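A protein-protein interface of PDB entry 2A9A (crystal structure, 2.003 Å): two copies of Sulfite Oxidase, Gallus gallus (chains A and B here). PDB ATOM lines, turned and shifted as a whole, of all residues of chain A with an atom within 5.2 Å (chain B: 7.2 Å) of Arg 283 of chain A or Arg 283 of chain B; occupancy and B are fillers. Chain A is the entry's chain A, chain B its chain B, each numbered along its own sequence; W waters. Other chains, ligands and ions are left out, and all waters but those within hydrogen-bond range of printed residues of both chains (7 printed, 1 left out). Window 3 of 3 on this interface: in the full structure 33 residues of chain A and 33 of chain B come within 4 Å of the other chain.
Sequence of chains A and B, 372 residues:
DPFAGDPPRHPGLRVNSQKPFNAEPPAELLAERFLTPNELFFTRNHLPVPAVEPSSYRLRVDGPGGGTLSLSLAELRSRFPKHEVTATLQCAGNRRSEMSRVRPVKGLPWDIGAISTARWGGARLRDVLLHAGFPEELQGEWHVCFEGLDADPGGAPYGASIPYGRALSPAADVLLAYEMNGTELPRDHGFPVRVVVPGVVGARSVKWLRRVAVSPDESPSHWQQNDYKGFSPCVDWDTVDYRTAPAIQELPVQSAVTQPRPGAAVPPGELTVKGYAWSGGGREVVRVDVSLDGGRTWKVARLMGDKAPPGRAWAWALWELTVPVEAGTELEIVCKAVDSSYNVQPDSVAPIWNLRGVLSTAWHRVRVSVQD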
ATOM      1  N   GLU A 250      17.527 -21.801  18.311  1.00  0.00           N
ATOM      2  CA  GLU A 250      17.254 -22.107  19.713  1.00  0.00           C
ATOM      3  C   GLU A 250      17.573 -23.575  20.025  1.00  0.00           C
ATOM      4  O   GLU A 250      17.343 -24.457  19.194  1.00  0.00           O
ATOM      5  CB  GLU A 250      15.803 -21.793  20.103  1.00  0.00           C
ATOM      6  CG  GLU A 250      15.477 -20.329  20.008  1.00  0.00           C
ATOM      7  CD  GLU A 250      14.056 -20.019  20.361  1.00  0.00           C
ATOM      8  OE1 GLU A 250      13.284 -20.939  20.767  1.00  0.00           O
ATOM      9  OE2 GLU A 250      13.688 -18.813  20.272  1.00  0.00           O
ATOM     10  N   LEU A 251      18.005 -23.837  21.253  1.00  0.00           N
ATOM     11  CA  LEU A 251      18.372 -25.200  21.711  1.00  0.00           C
ATOM     12  C   LEU A 251      17.312 -25.770  22.624  1.00  0.00           C
ATOM     13  O   LEU A 251      16.562 -25.003  23.221  1.00  0.00           O
ATOM     14  CB  LEU A 251      19.713 -25.184  22.466  1.00  0.00           C
ATOM     15  CG  LEU A 251      20.944 -25.047  21.563  1.00  0.00           C
ATOM     16  CD1 LEU A 251      22.185 -24.832  22.403  1.00  0.00           C
ATOM     17  CD2 LEU A 251      21.156 -26.252  20.695  1.00  0.00           C
ATOM     18  N   SER A 279      17.662 -24.038  29.172  1.00  0.00           N
ATOM     19  CA  SER A 279      16.866 -24.274  27.987  1.00  0.00           C
ATOM     20  C   SER A 279      17.009 -23.096  27.007  1.00  0.00           C
ATOM     21  O   SER A 279      17.304 -21.952  27.424  1.00  0.00           O
ATOM     22  CB  SER A 279      15.411 -24.503  28.419  1.00  0.00           C
ATOM     23  OG  SER A 279      14.626 -24.876  27.302  1.00  0.00           O
ATOM     24  N   GLY A 280      16.825 -23.327  25.710  1.00  0.00           N
ATOM     25  CA  GLY A 280      17.031 -22.224  24.781  1.00  0.00           C
ATOM     26  C   GLY A 280      15.864 -21.281  24.714  1.00  0.00           C
ATOM     27  O   GLY A 280      14.842 -21.458  25.379  1.00  0.00           O
ATOM     28  N   GLY A 281      16.022 -20.273  23.863  1.00  0.00           N
ATOM     29  CA  GLY A 281      14.942 -19.370  23.555  1.00  0.00           C
ATOM     30  C   GLY A 281      14.464 -18.514  24.689  1.00  0.00           C
ATOM     31  O   GLY A 281      13.385 -17.914  24.588  1.00  0.00           O
ATOM     32  N   GLY A 282      15.243 -18.401  25.760  1.00  0.00           N
ATOM     33  CA  GLY A 282      14.789 -17.546  26.866  1.00  0.00           C
ATOM     34  C   GLY A 282      13.773 -18.198  27.793  1.00  0.00           C
ATOM     35  O   GLY A 282      13.210 -17.522  28.648  1.00  0.00           O
ATOM     36  N   ARG A 283      13.612 -19.515  27.670  1.00  0.00           N
ATOM     37  CA  ARG A 283      12.675 -20.289  28.465  1.00  0.00           C
ATOM     38  C   ARG A 283      13.340 -20.754  29.761  1.00  0.00           C
ATOM     39  O   ARG A 283      14.363 -21.483  29.745  1.00  0.00           O
ATOM     40  CB  ARG A 283      12.165 -21.491  27.681  1.00  0.00           C
ATOM     41  CG  ARG A 283      11.235 -21.101  26.539  1.00  0.00           C
ATOM     42  CD  ARG A 283      10.805 -22.311  25.734  1.00  0.00           C
ATOM     43  NE  ARG A 283      11.849 -22.911  24.903  1.00  0.00           N
ATOM     44  CZ  ARG A 283      12.131 -22.508  23.655  1.00  0.00           C
ATOM     45  NH1 ARG A 283      11.526 -21.458  23.117  1.00  0.00           N
ATOM     46  NH2 ARG A 283      13.047 -23.144  22.963  1.00  0.00           N
ATOM     47  N   GLU A 284      12.780 -20.309  30.881  1.00  0.00           N
ATOM     48  CA  GLU A 284      13.376 -20.656  32.171  1.00  0.00           C
ATOM     49  C   GLU A 284      13.164 -22.112  32.524  1.00  0.00           C
ATOM     50  O   GLU A 284      12.252 -22.766  32.023  1.00  0.00           O
ATOM     51  CB  GLU A 284      12.858 -19.766  33.315  1.00  0.00           C
ATOM     52  CG  GLU A 284      11.421 -19.868  33.571  1.00  0.00           C
ATOM     53  CD  GLU A 284      10.985 -19.146  34.836  1.00  0.00           C
ATOM     54  OE1 GLU A 284      11.850 -18.745  35.682  1.00  0.00           O
ATOM     55  OE2 GLU A 284       9.748 -19.045  35.019  1.00  0.00           O
ATOM     56  N   VAL A 285      14.036 -22.596  33.405  1.00  0.00           N
ATOM     57  CA  VAL A 285      13.946 -23.933  33.927  1.00  0.00           C
ATOM     58  C   VAL A 285      13.005 -23.805  35.119  1.00  0.00           C
ATOM     59  O   VAL A 285      13.278 -23.028  36.053  1.00  0.00           O
ATOM     60  CB  VAL A 285      15.275 -24.401  34.414  1.00  0.00           C
ATOM     61  CG1 VAL A 285      15.143 -25.701  35.198  1.00  0.00           C
ATOM     62  CG2 VAL A 285      16.244 -24.525  33.226  1.00  0.00           C
ATOM     63  N   GLY A 311      10.518 -14.943  29.405  1.00  0.00           N
ATOM     64  CA  GLY A 311      11.028 -15.101  28.051  1.00  0.00           C
ATOM     65  C   GLY A 311      12.451 -14.584  27.909  1.00  0.00           C
ATOM     66  O   GLY A 311      13.003 -14.627  26.813  1.00  0.00           O
ATOM     67  N   ALA A 313      15.118 -15.651  30.011  1.00  0.00           N
ATOM     68  CA  ALA A 313      15.952 -16.530  30.875  1.00  0.00           C
ATOM     69  C   ALA A 313      17.174 -17.074  30.107  1.00  0.00           C
ATOM     70  O   ALA A 313      17.247 -18.265  29.769  1.00  0.00           O
ATOM     71  CB  ALA A 313      15.116 -17.670  31.437  1.00  0.00           C
ATOM     72  N   ASP A 339      11.192 -27.007  31.220  1.00  0.00           N
ATOM     73  CA  ASP A 339      11.240 -25.571  30.996  1.00  0.00           C
ATOM     74  C   ASP A 339       9.863 -24.908  31.013  1.00  0.00           C
ATOM     75  O   ASP A 339       8.863 -25.577  31.336  1.00  0.00           O
ATOM     76  CB  ASP A 339      12.061 -25.204  29.750  1.00  0.00           C
ATOM     77  CG  ASP A 339      11.299 -25.387  28.446  1.00  0.00           C
ATOM     78  OD1 ASP A 339      10.079 -25.508  28.491  1.00  0.00           O
ATOM     79  OD2 ASP A 339      11.932 -25.316  27.366  1.00  0.00           O
ATOM     80  N   SER A 340       9.841 -23.577  30.769  1.00  0.00           N
ATOM     81  CA  SER A 340       8.604 -22.787  30.874  1.00  0.00           C
ATOM     82  C   SER A 340       7.494 -23.179  29.907  1.00  0.00           C
ATOM     83  O   SER A 340       6.352 -22.880  30.193  1.00  0.00           O
ATOM     84  CB  SER A 340       8.875 -21.265  30.775  1.00  0.00           C
ATOM     85  OG  SER A 340       9.617 -20.931  29.630  1.00  0.00           O
ATOM     86  N   SER A 341       7.818 -23.763  28.744  1.00  0.00           N
ATOM     87  CA  SER A 341       6.782 -24.366  27.838  1.00  0.00           C
ATOM     88  C   SER A 341       6.498 -25.852  28.150  1.00  0.00           C
ATOM     89  O   SER A 341       5.956 -26.589  27.312  1.00  0.00           O
ATOM     90  CB  SER A 341       7.221 -24.287  26.373  1.00  0.00           C
ATOM     91  OG  SER A 341       8.525 -24.874  26.242  1.00  0.00           O
ATOM     92  N   ASN A 343       8.565 -28.229  28.082  1.00  0.00           N
ATOM     93  CA  ASN A 343       9.385 -29.159  27.339  1.00  0.00           C
ATOM     94  C   ASN A 343      10.249 -29.983  28.324  1.00  0.00           C
ATOM     95  O   ASN A 343      10.646 -29.473  29.364  1.00  0.00           O
ATOM     96  CB  ASN A 343      10.231 -28.461  26.290  1.00  0.00           C
ATOM     97  CG  ASN A 343       9.443 -28.175  25.012  1.00  0.00           C
ATOM     98  OD1 ASN A 343       8.968 -29.083  24.344  1.00  0.00           O
ATOM     99  ND2 ASN A 343       9.275 -26.901  24.701  1.00  0.00           N
ATOM    100  N   GLY B 199      -0.854 -21.073  20.024  1.00  0.00           N
ATOM    101  CA  GLY B 199       0.337 -21.717  20.573  1.00  0.00           C
ATOM    102  C   GLY B 199       0.307 -21.948  22.069  1.00  0.00           C
ATOM    103  O   GLY B 199       1.326 -22.363  22.659  1.00  0.00           O
ATOM    104  N   GLU B 250       2.367 -21.980  26.997  1.00  0.00           N
ATOM    105  CA  GLU B 250       2.843 -22.737  25.822  1.00  0.00           C
ATOM    106  C   GLU B 250       2.946 -24.246  26.166  1.00  0.00           C
ATOM    107  O   GLU B 250       3.343 -24.631  27.268  1.00  0.00           O
ATOM    108  CB  GLU B 250       4.216 -22.211  25.326  1.00  0.00           C
ATOM    109  CG  GLU B 250       4.169 -20.828  24.670  1.00  0.00           C
ATOM    110  CD  GLU B 250       5.557 -20.325  24.243  1.00  0.00           C
ATOM    111  OE1 GLU B 250       6.533 -21.128  24.266  1.00  0.00           O
ATOM    112  OE2 GLU B 250       5.668 -19.103  23.895  1.00  0.00           O
ATOM    113  N   LEU B 251       2.612 -25.089  25.185  1.00  0.00           N
ATOM    114  CA  LEU B 251       2.660 -26.540  25.305  1.00  0.00           C
ATOM    115  C   LEU B 251       3.867 -27.131  24.614  1.00  0.00           C
ATOM    116  O   LEU B 251       4.460 -26.519  23.766  1.00  0.00           O
ATOM    117  CB  LEU B 251       1.390 -27.128  24.671  1.00  0.00           C
ATOM    118  CG  LEU B 251       0.122 -27.045  25.538  1.00  0.00           C
ATOM    119  CD1 LEU B 251      -1.103 -27.505  24.756  1.00  0.00           C
ATOM    120  CD2 LEU B 251       0.259 -27.847  26.878  1.00  0.00           C
ATOM    121  N   PRO B 252       4.305 -28.306  25.054  1.00  0.00           N
ATOM    122  CA  PRO B 252       5.461 -28.958  24.440  1.00  0.00           C
ATOM    123  C   PRO B 252       5.110 -29.706  23.125  1.00  0.00           C
ATOM    124  O   PRO B 252       3.949 -29.850  22.782  1.00  0.00           O
ATOM    125  CB  PRO B 252       5.926 -29.910  25.556  1.00  0.00           C
ATOM    126  CG  PRO B 252       4.699 -30.204  26.292  1.00  0.00           C
ATOM    127  CD  PRO B 252       3.868 -28.996  26.275  1.00  0.00           C
ATOM    128  N   VAL B 253       6.123 -30.149  22.403  1.00  0.00           N
ATOM    129  CA  VAL B 253       5.952 -30.857  21.141  1.00  0.00           C
ATOM    130  C   VAL B 253       5.146 -32.154  21.364  1.00  0.00           C
ATOM    131  O   VAL B 253       5.294 -32.826  22.385  1.00  0.00           O
ATOM    132  CB  VAL B 253       7.297 -31.029  20.393  1.00  0.00           C
ATOM    133  CG1 VAL B 253       8.333 -31.797  21.218  1.00  0.00           C
ATOM    134  CG2 VAL B 253       7.078 -31.684  19.041  1.00  0.00           C
ATOM    135  N   TRP B 278       2.300 -31.318  16.430  1.00  0.00           N
ATOM    136  CA  TRP B 278       2.152 -29.899  16.732  1.00  0.00           C
ATOM    137  C   TRP B 278       3.033 -29.530  17.899  1.00  0.00           C
ATOM    138  O   TRP B 278       3.405 -30.404  18.681  1.00  0.00           O
ATOM    139  CB  TRP B 278       0.693 -29.594  17.078  1.00  0.00           C
ATOM    140  CG  TRP B 278       0.395 -28.180  17.474  1.00  0.00           C
ATOM    141  CD1 TRP B 278       0.128 -27.121  16.645  1.00  0.00           C
ATOM    142  CD2 TRP B 278       0.250 -27.687  18.808  1.00  0.00           C
ATOM    143  NE1 TRP B 278      -0.219 -26.015  17.389  1.00  0.00           N
ATOM    144  CE2 TRP B 278      -0.142 -26.333  18.716  1.00  0.00           C
ATOM    145  CE3 TRP B 278       0.421 -28.258  20.077  1.00  0.00           C
ATOM    146  CZ2 TRP B 278      -0.341 -25.537  19.839  1.00  0.00           C
ATOM    147  CZ3 TRP B 278       0.222 -27.461  21.190  1.00  0.00           C
ATOM    148  CH2 TRP B 278      -0.171 -26.123  21.065  1.00  0.00           C
ATOM    149  N   SER B 279       3.453 -28.266  17.945  1.00  0.00           N
ATOM    150  CA  SER B 279       4.204 -27.751  19.066  1.00  0.00           C
ATOM    151  C   SER B 279       3.674 -26.372  19.445  1.00  0.00           C
ATOM    152  O   SER B 279       3.075 -25.636  18.626  1.00  0.00           O
ATOM    153  CB  SER B 279       5.686 -27.706  18.734  1.00  0.00           C
ATOM    154  OG  SER B 279       6.449 -27.531  19.889  1.00  0.00           O
ATOM    155  N   GLY B 280       3.902 -26.018  20.697  1.00  0.00           N
ATOM    156  CA  GLY B 280       3.448 -24.762  21.255  1.00  0.00           C
ATOM    157  C   GLY B 280       4.388 -23.622  20.929  1.00  0.00           C
ATOM    158  O   GLY B 280       5.443 -23.811  20.317  1.00  0.00           O
ATOM    159  N   GLY B 281       3.935 -22.422  21.266  1.00  0.00           N
ATOM    160  CA  GLY B 281       4.702 -21.190  21.086  1.00  0.00           C
ATOM    161  C   GLY B 281       5.059 -20.742  19.684  1.00  0.00           C
ATOM    162  O   GLY B 281       5.991 -19.976  19.521  1.00  0.00           O
ATOM    163  N   GLY B 282       4.291 -21.157  18.682  1.00  0.00           N
ATOM    164  CA  GLY B 282       4.588 -20.808  17.280  1.00  0.00           C
ATOM    165  C   GLY B 282       5.724 -21.578  16.625  1.00  0.00           C
ATOM    166  O   GLY B 282       6.167 -21.215  15.508  1.00  0.00           O
ATOM    167  N   ARG B 283       6.197 -22.626  17.326  1.00  0.00           N
ATOM    168  CA  ARG B 283       7.282 -23.477  16.884  1.00  0.00           C
ATOM    169  C   ARG B 283       6.818 -24.531  15.901  1.00  0.00           C
ATOM    170  O   ARG B 283       6.038 -25.398  16.226  1.00  0.00           O
ATOM    171  CB  ARG B 283       7.976 -24.143  18.082  1.00  0.00           C
ATOM    172  CG  ARG B 283       8.694 -23.124  19.042  1.00  0.00           C
ATOM    173  CD  ARG B 283       9.535 -23.811  20.106  1.00  0.00           C
ATOM    174  NE  ARG B 283       8.726 -24.450  21.128  1.00  0.00           N
ATOM    175  CZ  ARG B 283       8.076 -23.818  22.114  1.00  0.00           C
ATOM    176  NH1 ARG B 283       8.130 -22.500  22.249  1.00  0.00           N
ATOM    177  NH2 ARG B 283       7.323 -24.544  22.934  1.00  0.00           N
ATOM    178  N   GLU B 284       7.346 -24.486  14.685  1.00  0.00           N
ATOM    179  CA  GLU B 284       6.927 -25.457  13.682  1.00  0.00           C
ATOM    180  C   GLU B 284       7.530 -26.822  13.969  1.00  0.00           C
ATOM    181  O   GLU B 284       8.518 -26.951  14.702  1.00  0.00           O
ATOM    182  CB  GLU B 284       7.233 -24.997  12.244  1.00  0.00           C
ATOM    183  CG  GLU B 284       8.639 -24.621  11.961  1.00  0.00           C
ATOM    184  CD  GLU B 284       8.932 -24.538  10.429  1.00  0.00           C
ATOM    185  OE1 GLU B 284       7.972 -24.280   9.629  1.00  0.00           O
ATOM    186  OE2 GLU B 284      10.120 -24.818  10.056  1.00  0.00           O
ATOM    187  N   VAL B 285       6.839 -27.830  13.451  1.00  0.00           N
ATOM    188  CA  VAL B 285       7.278 -29.215  13.480  1.00  0.00           C
ATOM    189  C   VAL B 285       8.203 -29.387  12.269  1.00  0.00           C
ATOM    190  O   VAL B 285       7.840 -29.037  11.134  1.00  0.00           O
ATOM    191  CB  VAL B 285       6.073 -30.181  13.378  1.00  0.00           C
ATOM    192  CG1 VAL B 285       6.549 -31.625  13.187  1.00  0.00           C
ATOM    193  CG2 VAL B 285       5.231 -30.099  14.636  1.00  0.00           C
ATOM    194  N   VAL B 286       9.442 -29.765  12.523  1.00  0.00           N
ATOM    195  CA  VAL B 286      10.425 -29.882  11.456  1.00  0.00           C
ATOM    196  C   VAL B 286      10.650 -31.313  11.006  1.00  0.00           C
ATOM    197  O   VAL B 286      11.293 -31.525  10.008  1.00  0.00           O
ATOM    198  CB  VAL B 286      11.782 -29.200  11.815  1.00  0.00           C
ATOM    199  CG1 VAL B 286      11.511 -27.762  12.258  1.00  0.00           C
ATOM    200  CG2 VAL B 286      12.520 -29.948  12.846  1.00  0.00           C
ATOM    201  N   PRO B 310       8.195 -17.551  10.456  1.00  0.00           N
ATOM    202  CA  PRO B 310       8.945 -17.975  11.657  1.00  0.00           C
ATOM    203  C   PRO B 310       8.227 -17.530  12.903  1.00  0.00           C
ATOM    204  O   PRO B 310       7.592 -16.496  12.864  1.00  0.00           O
ATOM    205  CB  PRO B 310      10.305 -17.263  11.544  1.00  0.00           C
ATOM    206  CG  PRO B 310      10.278 -16.481  10.281  1.00  0.00           C
ATOM    207  CD  PRO B 310       9.042 -16.841   9.481  1.00  0.00           C
ATOM    208  N   GLY B 311       8.187 -18.394  13.925  1.00  0.00           N
ATOM    209  CA  GLY B 311       7.549 -18.087  15.204  1.00  0.00           C
ATOM    210  C   GLY B 311       6.036 -18.041  15.197  1.00  0.00           C
ATOM    211  O   GLY B 311       5.423 -17.782  16.235  1.00  0.00           O
ATOM    212  N   ARG B 312       5.416 -18.339  14.055  1.00  0.00           N
ATOM    213  CA  ARG B 312       3.956 -18.234  13.945  1.00  0.00           C
ATOM    214  C   ARG B 312       3.287 -19.476  13.362  1.00  0.00           C
ATOM    215  O   ARG B 312       2.236 -19.394  12.727  1.00  0.00           O
ATOM    216  CB  ARG B 312       3.601 -16.935  13.228  1.00  0.00           C
ATOM    217  CG  ARG B 312       4.073 -15.722  14.068  1.00  0.00           C
ATOM    218  CD  ARG B 312       3.992 -14.437  13.337  1.00  0.00           C
ATOM    219  NE  ARG B 312       2.627 -14.309  12.905  1.00  0.00           N
ATOM    220  CZ  ARG B 312       2.212 -13.580  11.885  1.00  0.00           C
ATOM    221  NH1 ARG B 312       3.072 -12.854  11.169  1.00  0.00           N
ATOM    222  NH2 ARG B 312       0.915 -13.628  11.545  1.00  0.00           N
ATOM    223  N   ALA B 313       3.876 -20.635  13.670  1.00  0.00           N
ATOM    224  CA  ALA B 313       3.316 -21.937  13.308  1.00  0.00           C
ATOM    225  C   ALA B 313       2.303 -22.354  14.370  1.00  0.00           C
ATOM    226  O   ALA B 313       2.567 -23.195  15.237  1.00  0.00           O
ATOM    227  CB  ALA B 313       4.404 -22.984  13.147  1.00  0.00           C
ATOM    228  N   TRP B 314       1.098 -21.828  14.235  1.00  0.00           N
ATOM    229  CA  TRP B 314       0.050 -22.064  15.233  1.00  0.00           C
ATOM    230  C   TRP B 314      -0.768 -23.297  14.960  1.00  0.00           C
ATOM    231  O   TRP B 314      -1.517 -23.749  15.846  1.00  0.00           O
ATOM    232  CB  TRP B 314      -0.913 -20.872  15.300  1.00  0.00           C
ATOM    233  CG  TRP B 314      -0.309 -19.494  15.341  1.00  0.00           C
ATOM    234  CD1 TRP B 314      -0.605 -18.452  14.490  1.00  0.00           C
ATOM    235  CD2 TRP B 314       0.567 -18.942  16.334  1.00  0.00           C
ATOM    236  NE1 TRP B 314       0.072 -17.329  14.866  1.00  0.00           N
ATOM    237  CE2 TRP B 314       0.771 -17.580  16.003  1.00  0.00           C
ATOM    238  CE3 TRP B 314       1.188 -19.453  17.473  1.00  0.00           C
ATOM    239  CZ2 TRP B 314       1.572 -16.741  16.757  1.00  0.00           C
ATOM    240  CZ3 TRP B 314       1.994 -18.605  18.224  1.00  0.00           C
ATOM    241  CH2 TRP B 314       2.202 -17.286  17.851  1.00  0.00           C
ATOM    242  N   ALA B 315      -0.695 -23.798  13.718  1.00  0.00           N
ATOM    243  CA  ALA B 315      -1.480 -24.910  13.322  1.00  0.00           C
ATOM    244  C   ALA B 315      -0.661 -26.199  13.259  1.00  0.00           C
ATOM    245  O   ALA B 315       0.564 -26.182  13.079  1.00  0.00           O
ATOM    246  CB  ALA B 315      -2.135 -24.625  11.991  1.00  0.00           C
ATOM    247  N   VAL B 338       9.761 -33.477  16.224  1.00  0.00           N
ATOM    248  CA  VAL B 338      10.825 -32.570  16.599  1.00  0.00           C
ATOM    249  C   VAL B 338      10.380 -31.200  16.193  1.00  0.00           C
ATOM    250  O   VAL B 338       9.876 -31.051  15.098  1.00  0.00           O
ATOM    251  CB  VAL B 338      12.151 -32.912  15.859  1.00  0.00           C
ATOM    252  CG1 VAL B 338      13.278 -31.917  16.286  1.00  0.00           C
ATOM    253  CG2 VAL B 338      12.533 -34.360  16.120  1.00  0.00           C
ATOM    254  N   ASP B 339      10.523 -30.195  17.051  1.00  0.00           N
ATOM    255  CA  ASP B 339      10.108 -28.806  16.656  1.00  0.00           C
ATOM    256  C   ASP B 339      11.297 -27.919  16.197  1.00  0.00           C
ATOM    257  O   ASP B 339      12.435 -28.415  16.045  1.00  0.00           O
ATOM    258  CB  ASP B 339       9.169 -28.145  17.693  1.00  0.00           C
ATOM    259  CG  ASP B 339       9.885 -27.577  18.957  1.00  0.00           C
ATOM    260  OD1 ASP B 339      11.121 -27.448  19.011  1.00  0.00           O
ATOM    261  OD2 ASP B 339       9.146 -27.222  19.897  1.00  0.00           O
ATOM    262  N   SER B 340      11.030 -26.632  15.935  1.00  0.00           N
ATOM    263  CA  SER B 340      12.003 -25.710  15.361  1.00  0.00           C
ATOM    264  C   SER B 340      13.112 -25.282  16.354  1.00  0.00           C
ATOM    265  O   SER B 340      14.151 -24.781  15.951  1.00  0.00           O
ATOM    266  CB  SER B 340      11.245 -24.494  14.790  1.00  0.00           C
ATOM    267  OG  SER B 340      10.553 -23.841  15.841  1.00  0.00           O
ATOM    268  N   SER B 341      12.898 -25.542  17.648  1.00  0.00           N
ATOM    269  CA  SER B 341      13.896 -25.354  18.691  1.00  0.00           C
ATOM    270  C   SER B 341      14.556 -26.709  19.036  1.00  0.00           C
ATOM    271  O   SER B 341      15.263 -26.829  20.017  1.00  0.00           O
ATOM    272  CB  SER B 341      13.237 -24.811  19.951  1.00  0.00           C
ATOM    273  OG  SER B 341      14.212 -24.784  21.010  1.00  0.00           O
ATOM    274  N   TYR B 342      14.265 -27.718  18.227  1.00  0.00           N
ATOM    275  CA  TYR B 342      14.736 -29.082  18.371  1.00  0.00           C
ATOM    276  C   TYR B 342      14.314 -29.737  19.686  1.00  0.00           C
ATOM    277  O   TYR B 342      15.031 -30.562  20.220  1.00  0.00           O
ATOM    278  CB  TYR B 342      16.247 -29.186  18.082  1.00  0.00           C
ATOM    279  CG  TYR B 342      16.574 -29.198  16.590  1.00  0.00           C
ATOM    280  CD1 TYR B 342      16.541 -30.377  15.859  1.00  0.00           C
ATOM    281  CD2 TYR B 342      17.006 -28.038  15.937  1.00  0.00           C
ATOM    282  CE1 TYR B 342      16.858 -30.384  14.490  1.00  0.00           C
ATOM    283  CE2 TYR B 342      17.273 -28.018  14.576  1.00  0.00           C
ATOM    284  CZ  TYR B 342      17.240 -29.193  13.863  1.00  0.00           C
ATOM    285  OH  TYR B 342      17.617 -29.174  12.550  1.00  0.00           O
ATOM    286  N   ASN B 343      13.192 -29.294  20.253  1.00  0.00           N
ATOM    287  CA  ASN B 343      12.598 -29.995  21.393  1.00  0.00           C
ATOM    288  C   ASN B 343      11.987 -31.308  20.842  1.00  0.00           C
ATOM    289  O   ASN B 343      11.594 -31.384  19.674  1.00  0.00           O
ATOM    290  CB  ASN B 343      11.626 -29.101  22.179  1.00  0.00           C
ATOM    291  CG  ASN B 343      12.336 -28.337  23.315  1.00  0.00           C
ATOM    292  OD1 ASN B 343      12.794 -28.953  24.287  1.00  0.00           O
ATOM    293  ND2 ASN B 343      12.512 -27.019  23.160  1.00  0.00           N
HETATM  294  O   HOH W   1      14.821 -21.602  16.714  1.00  0.00           O
HETATM  295  O   HOH W   2       4.959 -20.490  28.155  1.00  0.00           O
HETATM  296  O   HOH W   3       3.760 -23.531  29.758  1.00  0.00           O
HETATM  297  O   HOH W   4      12.212 -22.131  17.923  1.00  0.00           O
HETATM  298  O   HOH W   5       8.928 -19.726  24.506  1.00  0.00           O
HETATM  299  O   HOH W   6       7.388 -20.562  27.386  1.00  0.00           O
HETATM  300  O   HOH W   7      16.819 -24.661  16.562  1.00  0.00           O
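O of Leu 251 of chain A sits at hydrogen-bond distance from OG of Ser 341 of chain B (3.2 Å). The guanidinium group of Arg 283 of chain A lies within hydrogen-bond range of the side-chain hydroxyl of Ser 341 of chain B (2.8 Å). O of Ser 341 of chain B sits close to O of Glu 250 of chain A (3.3 Å). The backbone carbonyl oxygen (O) of Glu 250 of chain B sits close to the backbone carbonyl oxygen (O) of Ser 341 of chain A (3.3 Å). O of Ser 341 of chain A sits close to N of Pro 252 of chain B (3.3 Å).
The side-chain hydroxyl (OG) of Ser 341 of chain A sits at hydrogen-bond distance from the side-chain carboxylate (OD1) of Asp 339 of chain A. OE1 of Glu 250 of chain B is in salt-bridge range of NH1 of Arg 283 of chain B (2.9 Å). The guanidinium group of Arg 283 of chain B lies close to the backbone carbonyl oxygen of Gly 280 of chain B (3.3 Å).
Arg 283 of chain A touches Arg 283 of chain B. Asn 343 of chain B touches Arg 283 of chain A (ND2 to NH2, 3.9 Å). C of Leu 251 of chain B touches O of Ser 341 of chain A (3.5 Å). Ser 341 of chain A touches Arg 283 of chain B (CB to NH2, 3.5 Å). Asn 343 of chain A touches Val 253 of chain B (OD1 to N, 3.6 Å). Asn 343 of chain A touches Arg 283 of chain B (ND2 to NH2, 3.5 Å). OD1 of Asn 343 of chain B touches CB of Asn 343 of chain A, at 3.3 Å.
Printed residues of chain B within 4 Å of Leu 251 of chain A: Ser 341. No residue of chain B comes within 4 Å of Gly 282 of chain A. Of the printed residues of chain B, Arg 283 of chain A touches Arg 283, Ser 341 and Asn 343. Of the printed residues of chain B, Ser 341 of chain A touches Glu 250 (3.3 Å), Leu 251 (3.5 Å), Pro 252 (3.3 Å) and Arg 283 (3.5 Å). Of the printed residues of chain A, Glu 250 of chain B touches Ser 341. Of the printed residues of chain A, Arg 283 of chain B touches Arg 283, Ser 341 and Asn 343.
Of the 15 printed residues of chain A, 5 touch a printed residue of chain B. Printed residues of chain B that touch a printed residue of chain A: Glu 250, Leu 251, Pro 252, Val 253, Arg 283, Ser 341 and Asn 343. Hydrophobic or aromatic side chains of chain B that line the printed part of chain A: Pro 252.
Glu 250 of chain A touches Ser 341 of chain B, and with the chains exchanged Ser 341 of chain A touches Glu 250 of chain B. Arg 283 of chain A touches its own counterpart, Arg 283 of chain B. Arg 283 of chain A touches Asn 343 of chain B, and with the chains exchanged Asn 343 of chain A touches Arg 283 of chain B. Positions printed for both chains: 250, 251, 279, 280, 281, 282, 283, 284, 285, 311, 313, 339, 340, 341 and 343.
Water W7 lies within hydrogen-bond range of O of Glu 250 of chain A (2.7 Å) and O of Ser 340 of chain B (2.7 Å). Water W5 bridges OE1 of Glu 250 of chain B (2.8 Å) and NH1 of Arg 283 of chain A (3.4 Å). Water W2 lies within hydrogen-bond range of the backbone NH of Glu 250 of chain B and the backbone carbonyl oxygen of Ser 340 of chain A.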
